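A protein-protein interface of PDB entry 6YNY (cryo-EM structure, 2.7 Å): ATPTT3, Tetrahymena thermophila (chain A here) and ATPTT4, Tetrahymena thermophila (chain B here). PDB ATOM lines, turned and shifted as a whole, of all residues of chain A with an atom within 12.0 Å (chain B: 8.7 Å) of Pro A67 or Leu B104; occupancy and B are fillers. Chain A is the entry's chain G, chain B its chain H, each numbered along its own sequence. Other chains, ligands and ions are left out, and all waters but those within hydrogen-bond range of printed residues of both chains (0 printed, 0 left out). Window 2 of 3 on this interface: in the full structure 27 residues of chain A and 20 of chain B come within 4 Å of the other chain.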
ATOM      1  N   ARG A  57      -2.823 -38.000 -31.315  1.00  0.00           N
ATOM      2  CA  ARG A  57      -2.307 -36.962 -32.199  1.00  0.00           C
ATOM      3  C   ARG A  57      -0.856 -37.225 -32.566  1.00  0.00           C
ATOM      4  O   ARG A  57      -0.486 -37.213 -33.745  1.00  0.00           O
ATOM      5  CB  ARG A  57      -2.443 -35.599 -31.527  1.00  0.00           C
ATOM      6  CG  ARG A  57      -2.077 -34.431 -32.409  1.00  0.00           C
ATOM      7  CD  ARG A  57      -2.022 -33.156 -31.613  1.00  0.00           C
ATOM      8  NE  ARG A  57      -0.961 -33.195 -30.619  1.00  0.00           N
ATOM      9  CZ  ARG A  57      -0.774 -32.267 -29.692  1.00  0.00           C
ATOM     10  NH1 ARG A  57       0.220 -32.386 -28.828  1.00  0.00           N
ATOM     11  NH2 ARG A  57      -1.578 -31.220 -29.627  1.00  0.00           N
ATOM     12  N   ASP A  58      -0.018 -37.463 -31.565  1.00  0.00           N
ATOM     13  CA  ASP A  58       1.397 -37.711 -31.765  1.00  0.00           C
ATOM     14  C   ASP A  58       1.759 -39.074 -31.200  1.00  0.00           C
ATOM     15  O   ASP A  58       1.110 -39.574 -30.277  1.00  0.00           O
ATOM     16  CB  ASP A  58       2.246 -36.633 -31.085  1.00  0.00           C
ATOM     17  CG  ASP A  58       1.784 -35.231 -31.415  1.00  0.00           C
ATOM     18  OD1 ASP A  58       1.286 -35.013 -32.538  1.00  0.00           O
ATOM     19  OD2 ASP A  58       1.916 -34.343 -30.547  1.00  0.00           O
ATOM     20  N   HIS A  61       5.575 -39.983 -26.645  1.00  0.00           N
ATOM     21  CA  HIS A  61       6.747 -39.144 -26.470  1.00  0.00           C
ATOM     22  C   HIS A  61       7.809 -39.861 -25.652  1.00  0.00           C
ATOM     23  O   HIS A  61       7.512 -40.498 -24.638  1.00  0.00           O
ATOM     24  CB  HIS A  61       6.364 -37.834 -25.787  1.00  0.00           C
ATOM     25  CG  HIS A  61       5.475 -36.958 -26.609  1.00  0.00           C
ATOM     26  ND1 HIS A  61       5.236 -37.187 -27.947  1.00  0.00           N
ATOM     27  CD2 HIS A  61       4.769 -35.850 -26.286  1.00  0.00           C
ATOM     28  CE1 HIS A  61       4.420 -36.258 -28.410  1.00  0.00           C
ATOM     29  NE2 HIS A  61       4.123 -35.434 -27.422  1.00  0.00           N
ATOM     30  N   GLU A  63      10.332 -38.040 -24.418  1.00  0.00           N
ATOM     31  CA  GLU A  63      10.742 -37.033 -23.454  1.00  0.00           C
ATOM     32  C   GLU A  63       9.701 -35.928 -23.463  1.00  0.00           C
ATOM     33  O   GLU A  63       8.874 -35.836 -24.373  1.00  0.00           O
ATOM     34  CB  GLU A  63      12.134 -36.474 -23.768  1.00  0.00           C
ATOM     35  CG  GLU A  63      12.224 -35.658 -25.048  1.00  0.00           C
ATOM     36  CD  GLU A  63      12.096 -36.501 -26.297  1.00  0.00           C
ATOM     37  OE1 GLU A  63      12.348 -37.720 -26.221  1.00  0.00           O
ATOM     38  OE2 GLU A  63      11.744 -35.945 -27.357  1.00  0.00           O
ATOM     39  N   VAL A  64       9.750 -35.089 -22.431  1.00  0.00           N
ATOM     40  CA  VAL A  64       8.843 -33.954 -22.351  1.00  0.00           C
ATOM     41  C   VAL A  64       9.210 -32.948 -23.430  1.00  0.00           C
ATOM     42  O   VAL A  64      10.381 -32.576 -23.584  1.00  0.00           O
ATOM     43  CB  VAL A  64       8.891 -33.323 -20.954  1.00  0.00           C
ATOM     44  CG1 VAL A  64       7.974 -32.127 -20.883  1.00  0.00           C
ATOM     45  CG2 VAL A  64       8.508 -34.343 -19.910  1.00  0.00           C
ATOM     46  N   ARG A  65       8.213 -32.506 -24.182  1.00  0.00           N
ATOM     47  CA  ARG A  65       8.403 -31.621 -25.318  1.00  0.00           C
ATOM     48  C   ARG A  65       7.752 -30.271 -25.045  1.00  0.00           C
ATOM     49  O   ARG A  65       7.176 -30.030 -23.983  1.00  0.00           O
ATOM     50  CB  ARG A  65       7.836 -32.262 -26.584  1.00  0.00           C
ATOM     51  CG  ARG A  65       8.493 -33.579 -26.930  1.00  0.00           C
ATOM     52  CD  ARG A  65       7.868 -34.235 -28.135  1.00  0.00           C
ATOM     53  NE  ARG A  65       8.430 -35.561 -28.359  1.00  0.00           N
ATOM     54  CZ  ARG A  65       8.070 -36.367 -29.350  1.00  0.00           C
ATOM     55  NH1 ARG A  65       8.639 -37.557 -29.467  1.00  0.00           N
ATOM     56  NH2 ARG A  65       7.149 -35.983 -30.222  1.00  0.00           N
ATOM     57  N   LYS A  66       7.859 -29.389 -26.018  1.00  0.00           N
ATOM     58  CA  LYS A  66       7.318 -28.047 -25.928  1.00  0.00           C
ATOM     59  C   LYS A  66       6.015 -27.941 -26.701  1.00  0.00           C
ATOM     60  O   LYS A  66       5.759 -28.721 -27.622  1.00  0.00           O
ATOM     61  CB  LYS A  66       8.326 -27.036 -26.475  1.00  0.00           C
ATOM     62  CG  LYS A  66       9.685 -27.119 -25.823  1.00  0.00           C
ATOM     63  CD  LYS A  66      10.653 -26.099 -26.382  1.00  0.00           C
ATOM     64  CE  LYS A  66      10.962 -26.340 -27.847  1.00  0.00           C
ATOM     65  NZ  LYS A  66      11.493 -27.700 -28.101  1.00  0.00           N
ATOM     66  N   PRO A  67       5.160 -26.978 -26.352  1.00  0.00           N
ATOM     67  CA  PRO A  67       3.895 -26.833 -27.085  1.00  0.00           C
ATOM     68  C   PRO A  67       4.080 -26.633 -28.574  1.00  0.00           C
ATOM     69  O   PRO A  67       3.244 -27.094 -29.361  1.00  0.00           O
ATOM     70  CB  PRO A  67       3.254 -25.605 -26.427  1.00  0.00           C
ATOM     71  CG  PRO A  67       3.863 -25.531 -25.086  1.00  0.00           C
ATOM     72  CD  PRO A  67       5.261 -26.022 -25.240  1.00  0.00           C
ATOM     73  N   GLN A  68       5.149 -25.960 -28.987  1.00  0.00           N
ATOM     74  CA  GLN A  68       5.407 -25.737 -30.402  1.00  0.00           C
ATOM     75  C   GLN A  68       6.077 -26.926 -31.076  1.00  0.00           C
ATOM     76  O   GLN A  68       6.181 -26.938 -32.306  1.00  0.00           O
ATOM     77  CB  GLN A  68       6.267 -24.486 -30.591  1.00  0.00           C
ATOM     78  CG  GLN A  68       7.553 -24.462 -29.787  1.00  0.00           C
ATOM     79  CD  GLN A  68       7.375 -23.833 -28.421  1.00  0.00           C
ATOM     80  OE1 GLN A  68       6.272 -23.798 -27.880  1.00  0.00           O
ATOM     81  NE2 GLN A  68       8.461 -23.325 -27.861  1.00  0.00           N
ATOM     82  N   ASP A  69       6.529 -27.920 -30.310  1.00  0.00           N
ATOM     83  CA  ASP A  69       7.102 -29.113 -30.920  1.00  0.00           C
ATOM     84  C   ASP A  69       6.038 -29.933 -31.634  1.00  0.00           C
ATOM     85  O   ASP A  69       6.337 -30.612 -32.620  1.00  0.00           O
ATOM     86  CB  ASP A  69       7.803 -29.962 -29.863  1.00  0.00           C
ATOM     87  CG  ASP A  69       9.005 -29.269 -29.264  1.00  0.00           C
ATOM     88  OD1 ASP A  69       9.581 -28.389 -29.934  1.00  0.00           O
ATOM     89  OD2 ASP A  69       9.380 -29.608 -28.122  1.00  0.00           O
ATOM     90  N   SER A  70       4.803 -29.886 -31.149  1.00  0.00           N
ATOM     91  CA  SER A  70       3.680 -30.571 -31.766  1.00  0.00           C
ATOM     92  C   SER A  70       2.834 -29.581 -32.558  1.00  0.00           C
ATOM     93  O   SER A  70       3.032 -28.366 -32.505  1.00  0.00           O
ATOM     94  CB  SER A  70       2.831 -31.280 -30.710  1.00  0.00           C
ATOM     95  OG  SER A  70       2.378 -30.370 -29.730  1.00  0.00           O
ATOM     96  N   LYS A  71       1.875 -30.123 -33.298  1.00  0.00           N
ATOM     97  CA  LYS A  71       1.016 -29.347 -34.182  1.00  0.00           C
ATOM     98  C   LYS A  71      -0.407 -29.377 -33.642  1.00  0.00           C
ATOM     99  O   LYS A  71      -1.068 -30.420 -33.677  1.00  0.00           O
ATOM    100  CB  LYS A  71       1.083 -29.905 -35.601  1.00  0.00           C
ATOM    101  CG  LYS A  71       0.185 -29.212 -36.597  1.00  0.00           C
ATOM    102  CD  LYS A  71       0.568 -29.566 -38.025  1.00  0.00           C
ATOM    103  CE  LYS A  71       0.593 -31.067 -38.252  1.00  0.00           C
ATOM    104  NZ  LYS A  71       0.821 -31.415 -39.684  1.00  0.00           N
ATOM    105  N   ASP A  72      -0.873 -28.234 -33.145  1.00  0.00           N
ATOM    106  CA  ASP A  72      -2.248 -28.122 -32.692  1.00  0.00           C
ATOM    107  C   ASP A  72      -3.206 -28.335 -33.858  1.00  0.00           C
ATOM    108  O   ASP A  72      -2.849 -28.165 -35.027  1.00  0.00           O
ATOM    109  CB  ASP A  72      -2.491 -26.753 -32.065  1.00  0.00           C
ATOM    110  CG  ASP A  72      -1.551 -26.463 -30.914  1.00  0.00           C
ATOM    111  OD1 ASP A  72      -1.173 -27.412 -30.196  1.00  0.00           O
ATOM    112  OD2 ASP A  72      -1.190 -25.282 -30.725  1.00  0.00           O
ATOM    113  N   VAL A  73      -4.437 -28.710 -33.524  1.00  0.00           N
ATOM    114  CA  VAL A  73      -5.522 -28.853 -34.495  1.00  0.00           C
ATOM    115  C   VAL A  73      -4.985 -29.543 -35.741  1.00  0.00           C
ATOM    116  O   VAL A  73      -4.850 -28.903 -36.793  1.00  0.00           O
ATOM    117  CB  VAL A  73      -6.185 -27.510 -34.837  1.00  0.00           C
ATOM    118  CG1 VAL A  73      -7.086 -27.081 -33.699  1.00  0.00           C
ATOM    119  CG2 VAL A  73      -5.161 -26.433 -35.154  1.00  0.00           C
ATOM    120  N   PRO A  74      -4.647 -30.825 -35.663  1.00  0.00           N
ATOM    121  CA  PRO A  74      -3.983 -31.488 -36.779  1.00  0.00           C
ATOM    122  C   PRO A  74      -4.755 -31.309 -38.070  1.00  0.00           C
ATOM    123  O   PRO A  74      -5.934 -30.923 -38.056  1.00  0.00           O
ATOM    124  CB  PRO A  74      -3.957 -32.961 -36.351  1.00  0.00           C
ATOM    125  CG  PRO A  74      -4.984 -33.081 -35.306  1.00  0.00           C
ATOM    126  CD  PRO A  74      -5.034 -31.775 -34.612  1.00  0.00           C
ATOM    127  N   HIS B  98       2.668 -36.424 -21.722  1.00  0.00           N
ATOM    128  CA  HIS B  98       1.976 -35.635 -22.734  1.00  0.00           C
ATOM    129  C   HIS B  98       1.295 -34.408 -22.147  1.00  0.00           C
ATOM    130  O   HIS B  98       1.078 -33.427 -22.865  1.00  0.00           O
ATOM    131  CB  HIS B  98       0.952 -36.499 -23.468  1.00  0.00           C
ATOM    132  CG  HIS B  98       1.553 -37.433 -24.469  1.00  0.00           C
ATOM    133  ND1 HIS B  98       1.371 -37.281 -25.824  1.00  0.00           N
ATOM    134  CD2 HIS B  98       2.336 -38.527 -24.316  1.00  0.00           C
ATOM    135  CE1 HIS B  98       2.011 -38.242 -26.463  1.00  0.00           C
ATOM    136  NE2 HIS B  98       2.606 -39.012 -25.571  1.00  0.00           N
ATOM    137  N   CYS B  99       0.945 -34.436 -20.861  1.00  0.00           N
ATOM    138  CA  CYS B  99       0.379 -33.253 -20.227  1.00  0.00           C
ATOM    139  C   CYS B  99       1.454 -32.263 -19.804  1.00  0.00           C
ATOM    140  O   CYS B  99       1.193 -31.055 -19.763  1.00  0.00           O
ATOM    141  CB  CYS B  99      -0.463 -33.655 -19.018  1.00  0.00           C
ATOM    142  SG  CYS B  99      -2.056 -34.379 -19.423  1.00  0.00           S
ATOM    143  N   LYS B 100       2.658 -32.745 -19.494  1.00  0.00           N
ATOM    144  CA  LYS B 100       3.754 -31.863 -19.120  1.00  0.00           C
ATOM    145  C   LYS B 100       4.251 -31.017 -20.279  1.00  0.00           C
ATOM    146  O   LYS B 100       5.003 -30.065 -20.050  1.00  0.00           O
ATOM    147  CB  LYS B 100       4.912 -32.677 -18.558  1.00  0.00           C
ATOM    148  CG  LYS B 100       4.669 -33.214 -17.171  1.00  0.00           C
ATOM    149  CD  LYS B 100       5.814 -34.084 -16.719  1.00  0.00           C
ATOM    150  CE  LYS B 100       5.516 -34.747 -15.394  1.00  0.00           C
ATOM    151  NZ  LYS B 100       6.590 -35.694 -15.011  1.00  0.00           N
ATOM    152  N   GLN B 101       3.856 -31.341 -21.509  1.00  0.00           N
ATOM    153  CA  GLN B 101       4.270 -30.542 -22.651  1.00  0.00           C
ATOM    154  C   GLN B 101       3.777 -29.109 -22.542  1.00  0.00           C
ATOM    155  O   GLN B 101       4.406 -28.194 -23.084  1.00  0.00           O
ATOM    156  CB  GLN B 101       3.753 -31.181 -23.936  1.00  0.00           C
ATOM    157  CG  GLN B 101       4.018 -30.368 -25.179  1.00  0.00           C
ATOM    158  CD  GLN B 101       3.712 -31.119 -26.458  1.00  0.00           C
ATOM    159  OE1 GLN B 101       4.304 -30.853 -27.501  1.00  0.00           O
ATOM    160  NE2 GLN B 101       2.783 -32.057 -26.388  1.00  0.00           N
ATOM    161  N   TYR B 102       2.669 -28.892 -21.839  1.00  0.00           N
ATOM    162  CA  TYR B 102       2.015 -27.595 -21.786  1.00  0.00           C
ATOM    163  C   TYR B 102       2.108 -26.946 -20.410  1.00  0.00           C
ATOM    164  O   TYR B 102       1.364 -26.004 -20.123  1.00  0.00           O
ATOM    165  CB  TYR B 102       0.556 -27.740 -22.205  1.00  0.00           C
ATOM    166  CG  TYR B 102       0.376 -28.311 -23.587  1.00  0.00           C
ATOM    167  CD1 TYR B 102       0.536 -27.521 -24.709  1.00  0.00           C
ATOM    168  CD2 TYR B 102       0.043 -29.642 -23.771  1.00  0.00           C
ATOM    169  CE1 TYR B 102       0.374 -28.035 -25.966  1.00  0.00           C
ATOM    170  CE2 TYR B 102      -0.123 -30.162 -25.029  1.00  0.00           C
ATOM    171  CZ  TYR B 102       0.044 -29.355 -26.122  1.00  0.00           C
ATOM    172  OH  TYR B 102      -0.119 -29.868 -27.384  1.00  0.00           O
ATOM    173  N   PHE B 103       3.006 -27.427 -19.554  1.00  0.00           N
ATOM    174  CA  PHE B 103       3.224 -26.817 -18.252  1.00  0.00           C
ATOM    175  C   PHE B 103       4.338 -25.783 -18.261  1.00  0.00           C
ATOM    176  O   PHE B 103       4.473 -25.035 -17.289  1.00  0.00           O
ATOM    177  CB  PHE B 103       3.539 -27.892 -17.209  1.00  0.00           C
ATOM    178  CG  PHE B 103       2.397 -28.828 -16.930  1.00  0.00           C
ATOM    179  CD1 PHE B 103       1.121 -28.555 -17.383  1.00  0.00           C
ATOM    180  CD2 PHE B 103       2.605 -29.983 -16.207  1.00  0.00           C
ATOM    181  CE1 PHE B 103       0.086 -29.415 -17.123  1.00  0.00           C
ATOM    182  CE2 PHE B 103       1.571 -30.843 -15.947  1.00  0.00           C
ATOM    183  CZ  PHE B 103       0.311 -30.559 -16.405  1.00  0.00           C
ATOM    184  N   LEU B 104       5.129 -25.720 -19.329  1.00  0.00           N
ATOM    185  CA  LEU B 104       6.149 -24.689 -19.491  1.00  0.00           C
ATOM    186  C   LEU B 104       7.197 -24.749 -18.387  1.00  0.00           C
ATOM    187  O   LEU B 104       7.723 -23.721 -17.959  1.00  0.00           O
ATOM    188  CB  LEU B 104       5.510 -23.303 -19.542  1.00  0.00           C
ATOM    189  CG  LEU B 104       4.407 -23.148 -20.587  1.00  0.00           C
ATOM    190  CD1 LEU B 104       3.760 -21.788 -20.486  1.00  0.00           C
ATOM    191  CD2 LEU B 104       4.953 -23.381 -21.976  1.00  0.00           C
ATOM    192  N   GLY B 105       7.514 -25.953 -17.925  1.00  0.00           N
ATOM    193  CA  GLY B 105       8.528 -26.114 -16.910  1.00  0.00           C
ATOM    194  C   GLY B 105       8.119 -25.693 -15.522  1.00  0.00           C
ATOM    195  O   GLY B 105       8.982 -25.595 -14.645  1.00  0.00           O
ATOM    196  N   ASP B 106       6.837 -25.442 -15.287  1.00  0.00           N
ATOM    197  CA  ASP B 106       6.359 -25.079 -13.957  1.00  0.00           C
ATOM    198  C   ASP B 106       6.487 -26.303 -13.063  1.00  0.00           C
ATOM    199  O   ASP B 106       5.658 -27.214 -13.110  1.00  0.00           O
ATOM    200  CB  ASP B 106       4.920 -24.586 -14.024  1.00  0.00           C
ATOM    201  CG  ASP B 106       4.468 -23.928 -12.739  1.00  0.00           C
ATOM    202  OD1 ASP B 106       5.039 -24.242 -11.675  1.00  0.00           O
ATOM    203  OD2 ASP B 106       3.542 -23.093 -12.795  1.00  0.00           O
ATOM    204  N   LYS B 107       7.531 -26.325 -12.236  1.00  0.00           N
ATOM    205  CA  LYS B 107       7.795 -27.498 -11.413  1.00  0.00           C
ATOM    206  C   LYS B 107       6.669 -27.738 -10.418  1.00  0.00           C
ATOM    207  O   LYS B 107       6.248 -28.881 -10.207  1.00  0.00           O
ATOM    208  CB  LYS B 107       9.126 -27.333 -10.686  1.00  0.00           C
ATOM    209  CG  LYS B 107       9.671 -28.611 -10.105  1.00  0.00           C
ATOM    210  CD  LYS B 107      10.141 -29.549 -11.199  1.00  0.00           C
ATOM    211  CE  LYS B 107      10.767 -30.803 -10.632  1.00  0.00           C
ATOM    212  NZ  LYS B 107      11.153 -31.745 -11.710  1.00  0.00           N
ATOM    213  N   LEU B 109       3.604 -27.078 -10.749  1.00  0.00           N
ATOM    214  CA  LEU B 109       2.441 -27.613 -11.444  1.00  0.00           C
ATOM    215  C   LEU B 109       2.638 -29.077 -11.807  1.00  0.00           C
ATOM    216  O   LEU B 109       1.702 -29.877 -11.706  1.00  0.00           O
ATOM    217  CB  LEU B 109       2.159 -26.784 -12.693  1.00  0.00           C
ATOM    218  CG  LEU B 109       0.861 -27.065 -13.438  1.00  0.00           C
ATOM    219  CD1 LEU B 109      -0.337 -26.892 -12.531  1.00  0.00           C
ATOM    220  CD2 LEU B 109       0.770 -26.144 -14.627  1.00  0.00           C
ATOM    221  N   GLU B 110       3.848 -29.444 -12.229  1.00  0.00           N
ATOM    222  CA  GLU B 110       4.140 -30.841 -12.523  1.00  0.00           C
ATOM    223  C   GLU B 110       3.933 -31.713 -11.294  1.00  0.00           C
ATOM    224  O   GLU B 110       3.401 -32.823 -11.392  1.00  0.00           O
ATOM    225  CB  GLU B 110       5.572 -30.973 -13.032  1.00  0.00           C
ATOM    226  CG  GLU B 110       5.841 -30.226 -14.318  1.00  0.00           C
ATOM    227  CD  GLU B 110       7.311 -30.207 -14.686  1.00  0.00           C
ATOM    228  OE1 GLU B 110       8.139 -30.642 -13.859  1.00  0.00           O
ATOM    229  OE2 GLU B 110       7.637 -29.757 -15.805  1.00  0.00           O
ATOM    230  N   ASN B 156      -4.645 -32.434 -26.421  1.00  0.00           N
ATOM    231  CA  ASN B 156      -4.750 -31.281 -25.534  1.00  0.00           C
ATOM    232  C   ASN B 156      -6.168 -30.719 -25.533  1.00  0.00           C
ATOM    233  O   ASN B 156      -6.388 -29.516 -25.675  1.00  0.00           O
ATOM    234  CB  ASN B 156      -3.736 -30.205 -25.913  1.00  0.00           C
ATOM    235  CG  ASN B 156      -3.573 -29.161 -24.840  1.00  0.00           C
ATOM    236  OD1 ASN B 156      -3.731 -29.442 -23.654  1.00  0.00           O
ATOM    237  ND2 ASN B 156      -3.262 -27.942 -25.248  1.00  0.00           N
ATOM    238  N   TYR B 165      -5.035 -25.188 -16.926  1.00  0.00           N
ATOM    239  CA  TYR B 165      -4.501 -23.944 -17.467  1.00  0.00           C
ATOM    240  C   TYR B 165      -5.238 -22.740 -16.896  1.00  0.00           C
ATOM    241  O   TYR B 165      -4.615 -21.749 -16.504  1.00  0.00           O
ATOM    242  CB  TYR B 165      -4.600 -23.948 -18.989  1.00  0.00           C
ATOM    243  CG  TYR B 165      -4.020 -25.171 -19.651  1.00  0.00           C
ATOM    244  CD1 TYR B 165      -2.898 -25.795 -19.138  1.00  0.00           C
ATOM    245  CD2 TYR B 165      -4.602 -25.706 -20.787  1.00  0.00           C
ATOM    246  CE1 TYR B 165      -2.373 -26.912 -19.737  1.00  0.00           C
ATOM    247  CE2 TYR B 165      -4.082 -26.819 -21.391  1.00  0.00           C
ATOM    248  CZ  TYR B 165      -2.970 -27.421 -20.864  1.00  0.00           C
ATOM    249  OH  TYR B 165      -2.456 -28.536 -21.472  1.00  0.00           O
ATOM    250  N   ARG B 168      -4.403 -22.250 -13.169  1.00  0.00           N
ATOM    251  CA  ARG B 168      -3.038 -21.795 -12.936  1.00  0.00           C
ATOM    252  C   ARG B 168      -2.868 -20.332 -13.323  1.00  0.00           C
ATOM    253  O   ARG B 168      -2.238 -19.562 -12.591  1.00  0.00           O
ATOM    254  CB  ARG B 168      -2.060 -22.678 -13.704  1.00  0.00           C
ATOM    255  CG  ARG B 168      -0.609 -22.494 -13.318  1.00  0.00           C
ATOM    256  CD  ARG B 168      -0.373 -22.871 -11.878  1.00  0.00           C
ATOM    257  NE  ARG B 168       1.038 -22.877 -11.523  1.00  0.00           N
ATOM    258  CZ  ARG B 168       1.488 -22.996 -10.280  1.00  0.00           C
ATOM    259  NH1 ARG B 168       0.638 -23.114  -9.274  1.00  0.00           N
ATOM    260  NH2 ARG B 168       2.786 -22.994 -10.041  1.00  0.00           N
ATOM    261  N   ASN B 169      -3.416 -19.932 -14.470  1.00  0.00           N
ATOM    262  CA  ASN B 169      -3.326 -18.534 -14.877  1.00  0.00           C
ATOM    263  C   ASN B 169      -3.988 -17.619 -13.856  1.00  0.00           C
ATOM    264  O   ASN B 169      -3.485 -16.526 -13.574  1.00  0.00           O
ATOM    265  CB  ASN B 169      -3.956 -18.350 -16.254  1.00  0.00           C
ATOM    266  CG  ASN B 169      -3.032 -18.763 -17.371  1.00  0.00           C
ATOM    267  OD1 ASN B 169      -1.827 -18.535 -17.312  1.00  0.00           O
ATOM    268  ND2 ASN B 169      -3.593 -19.378 -18.399  1.00  0.00           N
ATOM    269  N   LEU B 172      -1.331 -17.447 -10.963  1.00  0.00           N
ATOM    270  CA  LEU B 172      -0.121 -16.676 -11.213  1.00  0.00           C
ATOM    271  C   LEU B 172      -0.411 -15.187 -11.293  1.00  0.00           C
ATOM    272  O   LEU B 172       0.428 -14.369 -10.899  1.00  0.00           O
ATOM    273  CB  LEU B 172       0.542 -17.155 -12.499  1.00  0.00           C
ATOM    274  CG  LEU B 172       0.977 -18.615 -12.488  1.00  0.00           C
ATOM    275  CD1 LEU B 172       1.462 -19.031 -13.850  1.00  0.00           C
ATOM    276  CD2 LEU B 172       2.054 -18.830 -11.455  1.00  0.00           C
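Among the printed residues, merely in contact across the chains: Arg A57 with Gln B101 (3.6 Å), His A61 with Gln B101 (3.8 Å), Val A64 with Lys B100 (3.7 Å), Pro A67 with Gln B101 (3.2 Å), Pro A67 with Tyr B102 (3.7 Å), Pro A67 with Leu B104 (3.9 Å) and Asp A72 with Tyr B102 (3.9 Å).
Printed residues of chain B within 4 Å of Arg A57: Gln B101 and Tyr B102.
Printed residues of chain B within 4 Å of Val A64: Lys B100.
Of the printed residues of chain B, Arg A65 touches Gln B101 (3.2 Å).
Of chain B, only Gln B101, Tyr B102 and Leu B104 come within 4 Å of Pro A67.
Of chain B, only Gln B101 (3.0 Å) and Tyr B102 (3.5 Å) come within 4 Å of Ser A70.
Of the printed residues of chain A, His B98 touches His A61.
Tyr B102 touches just these residues of chain A: Arg A57 (2.9 Å), Pro A67 (3.7 Å), Ser A70 (3.5 Å) and Asp A72 (3.9 Å).
No residue of chain A comes within 4 Å of Phe B103.
Of the printed residues of chain A, Leu B104 touches Pro A67.
No residue of chain A comes within 4 Å of Asp B106.
Glu B110 touches none of the printed residues of chain A.
Asn B169 touches none of the printed residues of chain A.
The nearest printed residue of chain B that does not touch Arg A65 is Lys B100 (4.5 Å).
Of the 17 printed residues of chain B, 5 touch a printed residue of chain A.
Hydrophobic or aromatic side chains of chain B that line the printed part of chain A: His B98, Tyr B102 and Leu B104.
Along chain B the printed residues that touch a printed residue of chain A span positions 98 to 104.
Printed residues of chain A that touch a printed residue of chain B: Arg A57, His A61, Val A64, Arg A65, Lys A66, Pro A67, Ser A70 and Asp A72.
Hydrophobic or aromatic side chains of chain A that line the printed part of chain B: His A61, Val A64 and Pro A67.
Among the printed residues, no Asp or Glu carboxylate lies within 4 Å of a Lys or Arg side-chain nitrogen of the other chain.
NH1 of Arg A57 sits at hydrogen-bond distance from OG of Ser A70, at 3.1 Å.
OD2 of Asp A58 is in salt-bridge range of NE of Arg A57 (3.1 Å).
The side-chain carboxylate of Asp A72 lies within salt-bridge range of the guanidinium group of Arg A57 (3.9 Å).
NH2 of Arg A65 lies within hydrogen-bond range of ND1 of His A61, 3.2 Å away.
OD1 of Asp A69 lies within salt-bridge range of NZ of Lys A66 (2.7 Å).
O of Pro A67 lies within hydrogen-bond range of OG of Ser A70, at 3.4 Å.
OH of Tyr B102 sits at hydrogen-bond distance from NH1 of Arg A57 (2.9 Å).
OG of Ser A70 sits at hydrogen-bond distance from OH of Tyr B102.
OG of Ser A70 lies within hydrogen-bond range of OE1 of Gln B101 (3.0 Å).
The backbone NH of His A61 sits at hydrogen-bond distance from a ring nitrogen (NE2) of His B98.
O of Gln B101 sits close to O of Arg A65 (3.4 Å).
The backbone carbonyl oxygen (O) of Lys A66 sits close to the side-chain amide oxygen (OE1) of Gln B101 (2.6 Å).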
